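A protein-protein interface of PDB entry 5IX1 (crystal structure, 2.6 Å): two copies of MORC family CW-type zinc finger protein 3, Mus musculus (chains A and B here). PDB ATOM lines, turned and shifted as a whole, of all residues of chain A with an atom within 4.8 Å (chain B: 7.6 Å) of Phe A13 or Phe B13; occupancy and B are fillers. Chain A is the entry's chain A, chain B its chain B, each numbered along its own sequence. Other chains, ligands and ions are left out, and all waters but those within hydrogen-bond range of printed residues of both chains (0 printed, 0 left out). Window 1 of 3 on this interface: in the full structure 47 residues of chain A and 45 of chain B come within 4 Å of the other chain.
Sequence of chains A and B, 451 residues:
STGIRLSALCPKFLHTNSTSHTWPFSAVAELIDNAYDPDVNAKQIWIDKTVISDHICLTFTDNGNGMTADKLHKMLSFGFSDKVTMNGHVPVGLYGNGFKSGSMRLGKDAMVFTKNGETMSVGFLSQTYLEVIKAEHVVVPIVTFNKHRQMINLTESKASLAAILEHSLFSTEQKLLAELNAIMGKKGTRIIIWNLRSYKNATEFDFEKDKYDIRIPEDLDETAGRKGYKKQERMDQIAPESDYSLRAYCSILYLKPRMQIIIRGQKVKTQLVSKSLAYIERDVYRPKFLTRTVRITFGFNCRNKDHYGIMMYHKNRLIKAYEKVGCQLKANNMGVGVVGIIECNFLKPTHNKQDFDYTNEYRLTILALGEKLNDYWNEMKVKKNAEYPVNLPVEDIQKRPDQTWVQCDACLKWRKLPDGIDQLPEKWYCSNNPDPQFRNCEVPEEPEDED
Among the printed residues, merely in contact across the chains: Thr A16 with His B351 (3.5 Å), Asn A97 with Phe B13 (3.5 Å), Leu A9 with Leu B9 (3.6 Å), Lys A12 with Gly B79 (3.6 Å), Cys A10 with Phe B80 (3.6 Å), Phe A13 with Asn B97 (3.6 Å), Gly A79 with Lys B12 (3.6 Å), Phe A78 with Leu B9 (3.7 Å), Leu A9 with Phe B78 (3.8 Å), Thr A16 with Asn B97 (3.8 Å), Phe A13 with Phe B78 (3.8 Å), Gly A79 with Phe B13 (3.8 Å), Phe A13 with Gly B79 (3.8 Å), Phe A78 with Phe B13 (3.8 Å), Phe A13 with Phe B13 (3.8 Å) and Asn A97 with Thr B16 (3.9 Å).
The backbone NH (N) of Cys A10 is in hydrogen-bond range of the backbone carbonyl oxygen (O) of Phe B78 (3.1 Å). The side-chain sulfur of Cys A10 sits at hydrogen-bond distance from the backbone carbonyl oxygen of Gly B79. The backbone carbonyl oxygen (O) of Tyr B95 is in hydrogen-bond range of the side-chain hydroxyl (OG1) of Thr A16, at 3.0 Å. N of Phe A78 lies within hydrogen-bond range of O of Ala B8 (2.8 Å). O of Phe A78 sits at hydrogen-bond distance from N of Cys B10 (3.0 Å). O of Gly A79 lies within hydrogen-bond range of SG of Cys B10, 3.5 Å away.
Of chain B, only Phe B13 (3.8 Å), Phe B78 (3.8 Å), Gly B79 (3.8 Å) and Asn B97 (3.6 Å) come within 4 Å of Phe A13. Of the printed residues of chain A, Cys B10 touches Phe A78 and Gly A79. Printed residues of chain A within 4 Å of Lys B12: Gly A79. Of the printed residues of chain A, Phe B13 touches Phe A13, Phe A78, Gly A79 and Asn A97. The nearest printed residue of chain A that does not touch Tyr B95 is Lys A12 (4.7 Å).
Of the 12 printed residues of chain A, 8 touch a printed residue of chain B. Printed residues of chain A that touch a printed residue of chain B: Leu A9, Cys A10, Lys A12, Phe A13, Thr A16, Phe A78, Gly A79 and Asn A97. Hydrophobic or aromatic side chains of chain B that line the printed part of chain A: Leu B9, Phe B13, Phe B80, Tyr B95 and His B351. Along chain B the printed residues that touch a printed residue of chain A span positions 8 to 351.
SG of Cys A10 sits close to N of Lys A12, at 3.6 Å. The side-chain amide nitrogen of Asn A17 lies within hydrogen-bond range of the side-chain amide oxygen of Asn A97, at 2.8 Å. The backbone carbonyl oxygen (O) of Leu B9 sits at hydrogen-bond distance from the backbone NH (N) of Val B138. The side-chain sulfur (SG) of Cys B10 sits close to the backbone NH (N) of Lys B12. The side-chain amide nitrogen (ND2) of Asn B17 lies close to the side-chain amide nitrogen (ND2) of Asn B97 (3.1 Å). O of Gly B96 lies within hydrogen-bond range of N of Gly B79, 3.0 Å away.
Leu B9 touches its own counterpart, Leu A9. Cys A10 touches Phe B78, and with the chains exchanged Phe A78 touches Cys B10. Phe A13 touches Gly B79, and with the chains exchanged Gly A79 touches Phe B13. Phe A13 touches Asn B97, and with the chains exchanged Asn A97 touches Phe B13.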
ATOM      1  N   LEU A   9     -33.611  26.599 -24.115  1.00  0.00           N
ATOM      2  CA  LEU A   9     -32.818  27.601 -23.422  1.00  0.00           C
ATOM      3  C   LEU A   9     -33.531  28.899 -23.396  1.00  0.00           C
ATOM      4  O   LEU A   9     -33.891  29.415 -24.406  1.00  0.00           O
ATOM      5  CB  LEU A   9     -31.518  27.832 -24.132  1.00  0.00           C
ATOM      6  CG  LEU A   9     -30.432  26.851 -23.797  1.00  0.00           C
ATOM      7  CD1 LEU A   9     -29.444  26.827 -24.928  1.00  0.00           C
ATOM      8  CD2 LEU A   9     -29.765  27.263 -22.515  1.00  0.00           C
ATOM      9  N   CYS A  10     -33.694  29.439 -22.216  1.00  0.00           N
ATOM     10  CA  CYS A  10     -34.388  30.673 -22.029  1.00  0.00           C
ATOM     11  C   CYS A  10     -33.321  31.708 -21.984  1.00  0.00           C
ATOM     12  O   CYS A  10     -32.246  31.439 -21.510  1.00  0.00           O
ATOM     13  CB  CYS A  10     -35.143  30.632 -20.709  1.00  0.00           C
ATOM     14  SG  CYS A  10     -35.930  32.145 -20.156  1.00  0.00           S
ATOM     15  N   PRO A  11     -33.670  32.957 -22.507  1.00  0.00           N
ATOM     16  CA  PRO A  11     -32.574  33.928 -22.486  1.00  0.00           C
ATOM     17  C   PRO A  11     -32.060  34.215 -21.099  1.00  0.00           C
ATOM     18  O   PRO A  11     -30.915  34.564 -20.946  1.00  0.00           O
ATOM     19  CB  PRO A  11     -33.185  35.181 -23.085  1.00  0.00           C
ATOM     20  CG  PRO A  11     -34.611  35.075 -22.825  1.00  0.00           C
ATOM     21  CD  PRO A  11     -34.845  33.672 -23.203  1.00  0.00           C
ATOM     22  N   LYS A  12     -32.899  34.094 -20.103  1.00  0.00           N
ATOM     23  CA  LYS A  12     -32.534  34.438 -18.751  1.00  0.00           C
ATOM     24  C   LYS A  12     -31.378  33.585 -18.294  1.00  0.00           C
ATOM     25  O   LYS A  12     -30.585  33.991 -17.482  1.00  0.00           O
ATOM     26  CB  LYS A  12     -33.742  34.244 -17.855  1.00  0.00           C
ATOM     27  CG  LYS A  12     -33.475  34.182 -16.372  1.00  0.00           C
ATOM     28  CD  LYS A  12     -34.763  33.978 -15.611  1.00  0.00           C
ATOM     29  CE  LYS A  12     -35.805  34.986 -16.026  1.00  0.00           C
ATOM     30  NZ  LYS A  12     -37.159  34.587 -15.606  1.00  0.00           N
ATOM     31  N   PHE A  13     -31.270  32.400 -18.842  1.00  0.00           N
ATOM     32  CA  PHE A  13     -30.248  31.480 -18.429  1.00  0.00           C
ATOM     33  C   PHE A  13     -28.889  32.078 -18.681  1.00  0.00           C
ATOM     34  O   PHE A  13     -27.924  31.699 -18.052  1.00  0.00           O
ATOM     35  CB  PHE A  13     -30.381  30.173 -19.179  1.00  0.00           C
ATOM     36  CG  PHE A  13     -29.382  29.147 -18.780  1.00  0.00           C
ATOM     37  CD1 PHE A  13     -29.377  28.624 -17.520  1.00  0.00           C
ATOM     38  CD2 PHE A  13     -28.463  28.698 -19.673  1.00  0.00           C
ATOM     39  CE1 PHE A  13     -28.455  27.686 -17.155  1.00  0.00           C
ATOM     40  CE2 PHE A  13     -27.537  27.761 -19.320  1.00  0.00           C
ATOM     41  CZ  PHE A  13     -27.538  27.247 -18.056  1.00  0.00           C
ATOM     42  N   LEU A  14     -28.801  32.996 -19.622  1.00  0.00           N
ATOM     43  CA  LEU A  14     -27.521  33.580 -19.951  1.00  0.00           C
ATOM     44  C   LEU A  14     -26.941  34.265 -18.756  1.00  0.00           C
ATOM     45  O   LEU A  14     -25.763  34.202 -18.547  1.00  0.00           O
ATOM     46  CB  LEU A  14     -27.643  34.579 -21.087  1.00  0.00           C
ATOM     47  CG  LEU A  14     -27.888  34.020 -22.464  1.00  0.00           C
ATOM     48  CD1 LEU A  14     -28.122  35.162 -23.406  1.00  0.00           C
ATOM     49  CD2 LEU A  14     -26.719  33.202 -22.911  1.00  0.00           C
ATOM     50  N   HIS A  15     -27.755  34.958 -17.992  1.00  0.00           N
ATOM     51  CA  HIS A  15     -27.290  35.514 -16.742  1.00  0.00           C
ATOM     52  C   HIS A  15     -26.945  34.457 -15.726  1.00  0.00           C
ATOM     53  O   HIS A  15     -25.985  34.562 -15.008  1.00  0.00           O
ATOM     54  CB  HIS A  15     -28.296  36.464 -16.145  1.00  0.00           C
ATOM     55  CG  HIS A  15     -27.843  37.072 -14.868  1.00  0.00           C
ATOM     56  ND1 HIS A  15     -26.542  37.009 -14.445  1.00  0.00           N
ATOM     57  CD2 HIS A  15     -28.515  37.739 -13.910  1.00  0.00           C
ATOM     58  CE1 HIS A  15     -26.423  37.629 -13.291  1.00  0.00           C
ATOM     59  NE2 HIS A  15     -27.608  38.077 -12.942  1.00  0.00           N
ATOM     60  N   THR A  16     -27.761  33.431 -15.679  1.00  0.00           N
ATOM     61  CA  THR A  16     -27.645  32.399 -14.695  1.00  0.00           C
ATOM     62  C   THR A  16     -26.346  31.684 -14.843  1.00  0.00           C
ATOM     63  O   THR A  16     -25.689  31.391 -13.890  1.00  0.00           O
ATOM     64  CB  THR A  16     -28.820  31.433 -14.839  1.00  0.00           C
ATOM     65  OG1 THR A  16     -30.009  32.112 -14.463  1.00  0.00           O
ATOM     66  CG2 THR A  16     -28.655  30.254 -13.972  1.00  0.00           C
ATOM     67  N   ASN A  17     -25.974  31.430 -16.070  1.00  0.00           N
ATOM     68  CA  ASN A  17     -24.744  30.725 -16.367  1.00  0.00           C
ATOM     69  C   ASN A  17     -23.509  31.494 -16.009  1.00  0.00           C
ATOM     70  O   ASN A  17     -22.436  30.967 -16.029  1.00  0.00           O
ATOM     71  CB  ASN A  17     -24.691  30.349 -17.828  1.00  0.00           C
ATOM     72  CG  ASN A  17     -23.742  29.219 -18.096  1.00  0.00           C
ATOM     73  OD1 ASN A  17     -23.804  28.202 -17.454  1.00  0.00           O
ATOM     74  ND2 ASN A  17     -22.872  29.385 -19.060  1.00  0.00           N
ATOM     75  N   PHE A  78     -24.247  25.768 -26.037  1.00  0.00           N
ATOM     76  CA  PHE A  78     -23.788  25.336 -24.735  1.00  0.00           C
ATOM     77  C   PHE A  78     -23.362  23.886 -24.705  1.00  0.00           C
ATOM     78  O   PHE A  78     -24.114  23.019 -25.031  1.00  0.00           O
ATOM     79  CB  PHE A  78     -24.892  25.531 -23.724  1.00  0.00           C
ATOM     80  CG  PHE A  78     -25.241  26.955 -23.454  1.00  0.00           C
ATOM     81  CD1 PHE A  78     -24.732  27.606 -22.372  1.00  0.00           C
ATOM     82  CD2 PHE A  78     -26.113  27.617 -24.255  1.00  0.00           C
ATOM     83  CE1 PHE A  78     -25.073  28.892 -22.103  1.00  0.00           C
ATOM     84  CE2 PHE A  78     -26.456  28.911 -23.994  1.00  0.00           C
ATOM     85  CZ  PHE A  78     -25.932  29.552 -22.918  1.00  0.00           C
ATOM     86  N   GLY A  79     -22.154  23.628 -24.258  1.00  0.00           N
ATOM     87  CA  GLY A  79     -21.660  22.280 -24.164  1.00  0.00           C
ATOM     88  C   GLY A  79     -20.897  21.635 -25.291  1.00  0.00           C
ATOM     89  O   GLY A  79     -20.499  20.503 -25.150  1.00  0.00           O
ATOM     90  N   ASN A  97     -18.546  25.690 -22.003  1.00  0.00           N
ATOM     91  CA  ASN A  97     -19.366  26.740 -21.448  1.00  0.00           C
ATOM     92  C   ASN A  97     -18.596  28.017 -21.233  1.00  0.00           C
ATOM     93  O   ASN A  97     -19.156  29.043 -20.974  1.00  0.00           O
ATOM     94  CB  ASN A  97     -19.982  26.243 -20.145  1.00  0.00           C
ATOM     95  CG  ASN A  97     -20.922  27.217 -19.533  1.00  0.00           C
ATOM     96  OD1 ASN A  97     -20.721  27.646 -18.436  1.00  0.00           O
ATOM     97  ND2 ASN A  97     -21.953  27.553 -20.230  1.00  0.00           N
ATOM     98  N   ALA B   8     -27.979  26.029 -28.987  1.00  0.00           N
ATOM     99  CA  ALA B   8     -28.164  24.611 -28.816  1.00  0.00           C
ATOM    100  C   ALA B   8     -27.539  24.071 -27.549  1.00  0.00           C
ATOM    101  O   ALA B   8     -26.585  24.617 -27.043  1.00  0.00           O
ATOM    102  CB  ALA B   8     -27.598  23.886 -30.006  1.00  0.00           C
ATOM    103  N   LEU B   9     -28.111  22.991 -27.035  1.00  0.00           N
ATOM    104  CA  LEU B   9     -27.622  22.339 -25.833  1.00  0.00           C
ATOM    105  C   LEU B   9     -27.119  20.989 -26.164  1.00  0.00           C
ATOM    106  O   LEU B   9     -27.802  20.188 -26.726  1.00  0.00           O
ATOM    107  CB  LEU B   9     -28.727  22.165 -24.826  1.00  0.00           C
ATOM    108  CG  LEU B   9     -29.107  23.393 -24.046  1.00  0.00           C
ATOM    109  CD1 LEU B   9     -30.544  23.296 -23.615  1.00  0.00           C
ATOM    110  CD2 LEU B   9     -28.208  23.497 -22.853  1.00  0.00           C
ATOM    111  N   CYS B  10     -25.908  20.731 -25.757  1.00  0.00           N
ATOM    112  CA  CYS B  10     -25.263  19.493 -26.033  1.00  0.00           C
ATOM    113  C   CYS B  10     -25.367  18.684 -24.778  1.00  0.00           C
ATOM    114  O   CYS B  10     -25.274  19.232 -23.697  1.00  0.00           O
ATOM    115  CB  CYS B  10     -23.816  19.779 -26.342  1.00  0.00           C
ATOM    116  SG  CYS B  10     -22.809  18.354 -26.662  1.00  0.00           S
ATOM    117  N   PRO B  11     -25.432  17.378 -24.902  1.00  0.00           N
ATOM    118  CA  PRO B  11     -25.650  16.502 -23.763  1.00  0.00           C
ATOM    119  C   PRO B  11     -24.565  16.683 -22.756  1.00  0.00           C
ATOM    120  O   PRO B  11     -24.804  16.586 -21.589  1.00  0.00           O
ATOM    121  CB  PRO B  11     -25.528  15.134 -24.383  1.00  0.00           C
ATOM    122  CG  PRO B  11     -26.093  15.316 -25.729  1.00  0.00           C
ATOM    123  CD  PRO B  11     -25.785  16.715 -26.157  1.00  0.00           C
ATOM    124  N   LYS B  12     -23.372  16.938 -23.217  1.00  0.00           N
ATOM    125  CA  LYS B  12     -22.231  17.038 -22.359  1.00  0.00           C
ATOM    126  C   LYS B  12     -22.439  18.159 -21.382  1.00  0.00           C
ATOM    127  O   LYS B  12     -21.875  18.171 -20.324  1.00  0.00           O
ATOM    128  CB  LYS B  12     -21.001  17.292 -23.209  1.00  0.00           C
ATOM    129  CG  LYS B  12     -19.816  17.847 -22.468  1.00  0.00           C
ATOM    130  CD  LYS B  12     -18.631  17.964 -23.382  1.00  0.00           C
ATOM    131  CE  LYS B  12     -18.358  16.657 -24.081  1.00  0.00           C
ATOM    132  NZ  LYS B  12     -17.933  16.861 -25.484  1.00  0.00           N
ATOM    133  N   PHE B  13     -23.248  19.120 -21.754  1.00  0.00           N
ATOM    134  CA  PHE B  13     -23.476  20.269 -20.913  1.00  0.00           C
ATOM    135  C   PHE B  13     -24.112  19.869 -19.606  1.00  0.00           C
ATOM    136  O   PHE B  13     -23.981  20.558 -18.623  1.00  0.00           O
ATOM    137  CB  PHE B  13     -24.334  21.298 -21.627  1.00  0.00           C
ATOM    138  CG  PHE B  13     -24.508  22.564 -20.867  1.00  0.00           C
ATOM    139  CD1 PHE B  13     -23.442  23.348 -20.560  1.00  0.00           C
ATOM    140  CD2 PHE B  13     -25.741  22.955 -20.457  1.00  0.00           C
ATOM    141  CE1 PHE B  13     -23.604  24.501 -19.855  1.00  0.00           C
ATOM    142  CE2 PHE B  13     -25.915  24.100 -19.746  1.00  0.00           C
ATOM    143  CZ  PHE B  13     -24.841  24.881 -19.448  1.00  0.00           C
ATOM    144  N   LEU B  14     -24.830  18.764 -19.598  1.00  0.00           N
ATOM    145  CA  LEU B  14     -25.529  18.351 -18.398  1.00  0.00           C
ATOM    146  C   LEU B  14     -24.561  18.124 -17.281  1.00  0.00           C
ATOM    147  O   LEU B  14     -24.828  18.488 -16.169  1.00  0.00           O
ATOM    148  CB  LEU B  14     -26.305  17.066 -18.637  1.00  0.00           C
ATOM    149  CG  LEU B  14     -27.578  17.206 -19.434  1.00  0.00           C
ATOM    150  CD1 LEU B  14     -28.137  15.851 -19.762  1.00  0.00           C
ATOM    151  CD2 LEU B  14     -28.570  18.011 -18.659  1.00  0.00           C
ATOM    152  N   HIS B  15     -23.438  17.507 -17.575  1.00  0.00           N
ATOM    153  CA  HIS B  15     -22.382  17.401 -16.603  1.00  0.00           C
ATOM    154  C   HIS B  15     -21.746  18.726 -16.250  1.00  0.00           C
ATOM    155  O   HIS B  15     -21.354  18.945 -15.140  1.00  0.00           O
ATOM    156  CB  HIS B  15     -21.328  16.399 -17.008  1.00  0.00           C
ATOM    157  CG  HIS B  15     -20.176  16.354 -16.071  1.00  0.00           C
ATOM    158  ND1 HIS B  15     -20.331  16.223 -14.716  1.00  0.00           N
ATOM    159  CD2 HIS B  15     -18.853  16.470 -16.283  1.00  0.00           C
ATOM    160  CE1 HIS B  15     -19.152  16.237 -14.134  1.00  0.00           C
ATOM    161  NE2 HIS B  15     -18.237  16.389 -15.064  1.00  0.00           N
ATOM    162  N   THR B  16     -21.587  19.580 -17.231  1.00  0.00           N
ATOM    163  CA  THR B  16     -20.952  20.858 -17.046  1.00  0.00           C
ATOM    164  C   THR B  16     -21.723  21.734 -16.109  1.00  0.00           C
ATOM    165  O   THR B  16     -21.164  22.396 -15.286  1.00  0.00           O
ATOM    166  CB  THR B  16     -20.774  21.547 -18.402  1.00  0.00           C
ATOM    167  OG1 THR B  16     -19.877  20.774 -19.185  1.00  0.00           O
ATOM    168  CG2 THR B  16     -20.220  22.904 -18.235  1.00  0.00           C
ATOM    169  N   ASN B  17     -23.027  21.710 -16.227  1.00  0.00           N
ATOM    170  CA  ASN B  17     -23.863  22.538 -15.405  1.00  0.00           C
ATOM    171  C   ASN B  17     -23.787  22.140 -13.956  1.00  0.00           C
ATOM    172  O   ASN B  17     -24.199  22.861 -13.088  1.00  0.00           O
ATOM    173  CB  ASN B  17     -25.285  22.475 -15.883  1.00  0.00           C
ATOM    174  CG  ASN B  17     -26.083  23.645 -15.432  1.00  0.00           C
ATOM    175  OD1 ASN B  17     -25.606  24.750 -15.447  1.00  0.00           O
ATOM    176  ND2 ASN B  17     -27.301  23.408 -15.028  1.00  0.00           N
ATOM    177  N   SER B  18     -23.299  20.950 -13.703  1.00  0.00           N
ATOM    178  CA  SER B  18     -23.267  20.428 -12.364  1.00  0.00           C
ATOM    179  C   SER B  18     -21.993  20.704 -11.632  1.00  0.00           C
ATOM    180  O   SER B  18     -21.820  20.255 -10.531  1.00  0.00           O
ATOM    181  CB  SER B  18     -23.540  18.935 -12.385  1.00  0.00           C
ATOM    182  OG  SER B  18     -22.371  18.169 -12.479  1.00  0.00           O
ATOM    183  N   THR B  19     -21.080  21.413 -12.254  1.00  0.00           N
ATOM    184  CA  THR B  19     -19.760  21.567 -11.693  1.00  0.00           C
ATOM    185  C   THR B  19     -19.614  22.652 -10.666  1.00  0.00           C
ATOM    186  O   THR B  19     -18.576  22.799 -10.113  1.00  0.00           O
ATOM    187  CB  THR B  19     -18.704  21.686 -12.776  1.00  0.00           C
ATOM    188  OG1 THR B  19     -19.237  22.402 -13.886  1.00  0.00           O
ATOM    189  CG2 THR B  19     -18.337  20.332 -13.247  1.00  0.00           C
ATOM    190  N   SER B  77     -35.923  22.129 -18.786  1.00  0.00           N
ATOM    191  CA  SER B  77     -35.350  23.114 -19.670  1.00  0.00           C
ATOM    192  C   SER B  77     -34.535  24.072 -18.843  1.00  0.00           C
ATOM    193  O   SER B  77     -34.713  24.137 -17.655  1.00  0.00           O
ATOM    194  CB  SER B  77     -36.457  23.866 -20.369  1.00  0.00           C
ATOM    195  OG  SER B  77     -36.922  23.128 -21.457  1.00  0.00           O
ATOM    196  N   PHE B  78     -33.649  24.829 -19.462  1.00  0.00           N
ATOM    197  CA  PHE B  78     -32.724  25.633 -18.698  1.00  0.00           C
ATOM    198  C   PHE B  78     -33.095  27.099 -18.674  1.00  0.00           C
ATOM    199  O   PHE B  78     -33.236  27.710 -19.690  1.00  0.00           O
ATOM    200  CB  PHE B  78     -31.334  25.491 -19.274  1.00  0.00           C
ATOM    201  CG  PHE B  78     -30.762  24.120 -19.171  1.00  0.00           C
ATOM    202  CD1 PHE B  78     -31.205  23.118 -19.968  1.00  0.00           C
ATOM    203  CD2 PHE B  78     -29.750  23.860 -18.306  1.00  0.00           C
ATOM    204  CE1 PHE B  78     -30.664  21.869 -19.885  1.00  0.00           C
ATOM    205  CE2 PHE B  78     -29.196  22.623 -18.225  1.00  0.00           C
ATOM    206  CZ  PHE B  78     -29.657  21.622 -19.013  1.00  0.00           C
ATOM    207  N   GLY B  79     -33.210  27.666 -17.492  1.00  0.00           N
ATOM    208  CA  GLY B  79     -33.532  29.062 -17.333  1.00  0.00           C
ATOM    209  C   GLY B  79     -34.955  29.529 -17.179  1.00  0.00           C
ATOM    210  O   GLY B  79     -35.166  30.692 -16.931  1.00  0.00           O
ATOM    211  N   PHE B  80     -35.928  28.643 -17.269  1.00  0.00           N
ATOM    212  CA  PHE B  80     -37.309  29.064 -17.131  1.00  0.00           C
ATOM    213  C   PHE B  80     -37.744  29.002 -15.694  1.00  0.00           C
ATOM    214  O   PHE B  80     -37.783  27.955 -15.119  1.00  0.00           O
ATOM    215  CB  PHE B  80     -38.203  28.159 -17.930  1.00  0.00           C
ATOM    216  CG  PHE B  80     -37.927  28.178 -19.382  1.00  0.00           C
ATOM    217  CD1 PHE B  80     -38.681  28.937 -20.219  1.00  0.00           C
ATOM    218  CD2 PHE B  80     -36.916  27.434 -19.902  1.00  0.00           C
ATOM    219  CE1 PHE B  80     -38.432  28.954 -21.553  1.00  0.00           C
ATOM    220  CE2 PHE B  80     -36.661  27.445 -21.240  1.00  0.00           C
ATOM    221  CZ  PHE B  80     -37.424  28.206 -22.063  1.00  0.00           C
ATOM    222  N   TYR B  95     -33.175  31.613 -10.695  1.00  0.00           N
ATOM    223  CA  TYR B  95     -32.276  31.215 -11.758  1.00  0.00           C
ATOM    224  C   TYR B  95     -32.791  30.269 -12.822  1.00  0.00           C
ATOM    225  O   TYR B  95     -32.359  30.332 -13.927  1.00  0.00           O
ATOM    226  CB  TYR B  95     -30.973  30.712 -11.196  1.00  0.00           C
ATOM    227  CG  TYR B  95     -30.207  31.748 -10.452  1.00  0.00           C
ATOM    228  CD1 TYR B  95     -30.411  33.084 -10.671  1.00  0.00           C
ATOM    229  CD2 TYR B  95     -29.272  31.392  -9.534  1.00  0.00           C
ATOM    230  CE1 TYR B  95     -29.699  34.031  -9.986  1.00  0.00           C
ATOM    231  CE2 TYR B  95     -28.566  32.330  -8.847  1.00  0.00           C
ATOM    232  CZ  TYR B  95     -28.784  33.641  -9.083  1.00  0.00           C
ATOM    233  OH  TYR B  95     -28.080  34.538  -8.373  1.00  0.00           O
ATOM    234  N   GLY B  96     -33.644  29.331 -12.473  1.00  0.00           N
ATOM    235  CA  GLY B  96     -34.154  28.373 -13.431  1.00  0.00           C
ATOM    236  C   GLY B  96     -33.244  27.220 -13.734  1.00  0.00           C
ATOM    237  O   GLY B  96     -33.420  26.553 -14.706  1.00  0.00           O
ATOM    238  N   ASN B  97     -32.230  27.019 -12.922  1.00  0.00           N
ATOM    239  CA  ASN B  97     -31.241  26.002 -13.205  1.00  0.00           C
ATOM    240  C   ASN B  97     -31.107  24.920 -12.139  1.00  0.00           C
ATOM    241  O   ASN B  97     -30.497  23.905 -12.349  1.00  0.00           O
ATOM    242  CB  ASN B  97     -29.912  26.709 -13.453  1.00  0.00           C
ATOM    243  CG  ASN B  97     -28.809  25.784 -13.830  1.00  0.00           C
ATOM    244  OD1 ASN B  97     -28.905  25.031 -14.767  1.00  0.00           O
ATOM    245  ND2 ASN B  97     -27.739  25.862 -13.107  1.00  0.00           N
ATOM    246  N   GLY B  98     -31.725  25.122 -10.998  1.00  0.00           N
ATOM    247  CA  GLY B  98     -31.447  24.298  -9.844  1.00  0.00           C
ATOM    248  C   GLY B  98     -31.702  22.809  -9.911  1.00  0.00           C
ATOM    249  O   GLY B  98     -30.902  22.044  -9.417  1.00  0.00           O
ATOM    250  N   LYS B 100     -31.661  20.981 -12.644  1.00  0.00           N
ATOM    251  CA  LYS B 100     -30.713  20.394 -13.554  1.00  0.00           C
ATOM    252  C   LYS B 100     -29.380  20.314 -12.915  1.00  0.00           C
ATOM    253  O   LYS B 100     -28.706  19.318 -13.000  1.00  0.00           O
ATOM    254  CB  LYS B 100     -30.612  21.208 -14.828  1.00  0.00           C
ATOM    255  CG  LYS B 100     -31.882  21.264 -15.635  1.00  0.00           C
ATOM    256  CD  LYS B 100     -32.371  22.680 -15.734  1.00  0.00           C
ATOM    257  CE  LYS B 100     -33.779  22.811 -15.240  1.00  0.00           C
ATOM    258  NZ  LYS B 100     -33.834  23.774 -14.133  1.00  0.00           N
ATOM    259  N   MET B 104     -28.074  16.432 -11.714  1.00  0.00           N
ATOM    260  CA  MET B 104     -26.943  15.948 -12.437  1.00  0.00           C
ATOM    261  C   MET B 104     -25.708  15.865 -11.581  1.00  0.00           C
ATOM    262  O   MET B 104     -24.815  15.112 -11.842  1.00  0.00           O
ATOM    263  CB  MET B 104     -26.792  16.721 -13.718  1.00  0.00           C
ATOM    264  CG  MET B 104     -28.041  16.629 -14.560  1.00  0.00           C
ATOM    265  SD  MET B 104     -28.144  15.120 -15.503  1.00  0.00           S
ATOM    266  CE  MET B 104     -29.209  14.134 -14.505  1.00  0.00           C
ATOM    267  N   GLN B 127     -28.179  11.458 -18.748  1.00  0.00           N
ATOM    268  CA  GLN B 127     -26.930  11.464 -19.453  1.00  0.00           C
ATOM    269  C   GLN B 127     -26.684  10.149 -20.120  1.00  0.00           C
ATOM    270  O   GLN B 127     -26.142  10.098 -21.194  1.00  0.00           O
ATOM    271  CB  GLN B 127     -25.789  11.771 -18.516  1.00  0.00           C
ATOM    272  CG  GLN B 127     -25.595  13.244 -18.274  1.00  0.00           C
ATOM    273  CD  GLN B 127     -24.509  13.517 -17.289  1.00  0.00           C
ATOM    274  OE1 GLN B 127     -23.396  13.074 -17.448  1.00  0.00           O
ATOM    275  NE2 GLN B 127     -24.839  14.222 -16.251  1.00  0.00           N
ATOM    276  N   VAL B 138     -29.962  17.924 -26.374  1.00  0.00           N
ATOM    277  CA  VAL B 138     -30.595  17.405 -25.197  1.00  0.00           C
ATOM    278  C   VAL B 138     -32.067  17.305 -25.478  1.00  0.00           C
ATOM    279  O   VAL B 138     -32.743  18.284 -25.670  1.00  0.00           O
ATOM    280  CB  VAL B 138     -30.320  18.291 -23.983  1.00  0.00           C
ATOM    281  CG1 VAL B 138     -31.245  17.962 -22.832  1.00  0.00           C
ATOM    282  CG2 VAL B 138     -28.893  18.113 -23.543  1.00  0.00           C
ATOM    283  N   HIS B 351     -23.909  30.457  -8.006  1.00  0.00           N
ATOM    284  CA  HIS B 351     -24.427  29.422  -8.861  1.00  0.00           C
ATOM    285  C   HIS B 351     -24.945  28.231  -8.078  1.00  0.00           C
ATOM    286  O   HIS B 351     -25.911  27.607  -8.468  1.00  0.00           O
ATOM    287  CB  HIS B 351     -23.337  28.989  -9.828  1.00  0.00           C
ATOM    288  CG  HIS B 351     -23.838  28.261 -11.023  1.00  0.00           C
ATOM    289  ND1 HIS B 351     -23.480  26.969 -11.306  1.00  0.00           N
ATOM    290  CD2 HIS B 351     -24.663  28.645 -12.013  1.00  0.00           C
ATOM    291  CE1 HIS B 351     -24.067  26.587 -12.415  1.00  0.00           C
ATOM    292  NE2 HIS B 351     -24.789  27.587 -12.866  1.00  0.00           N
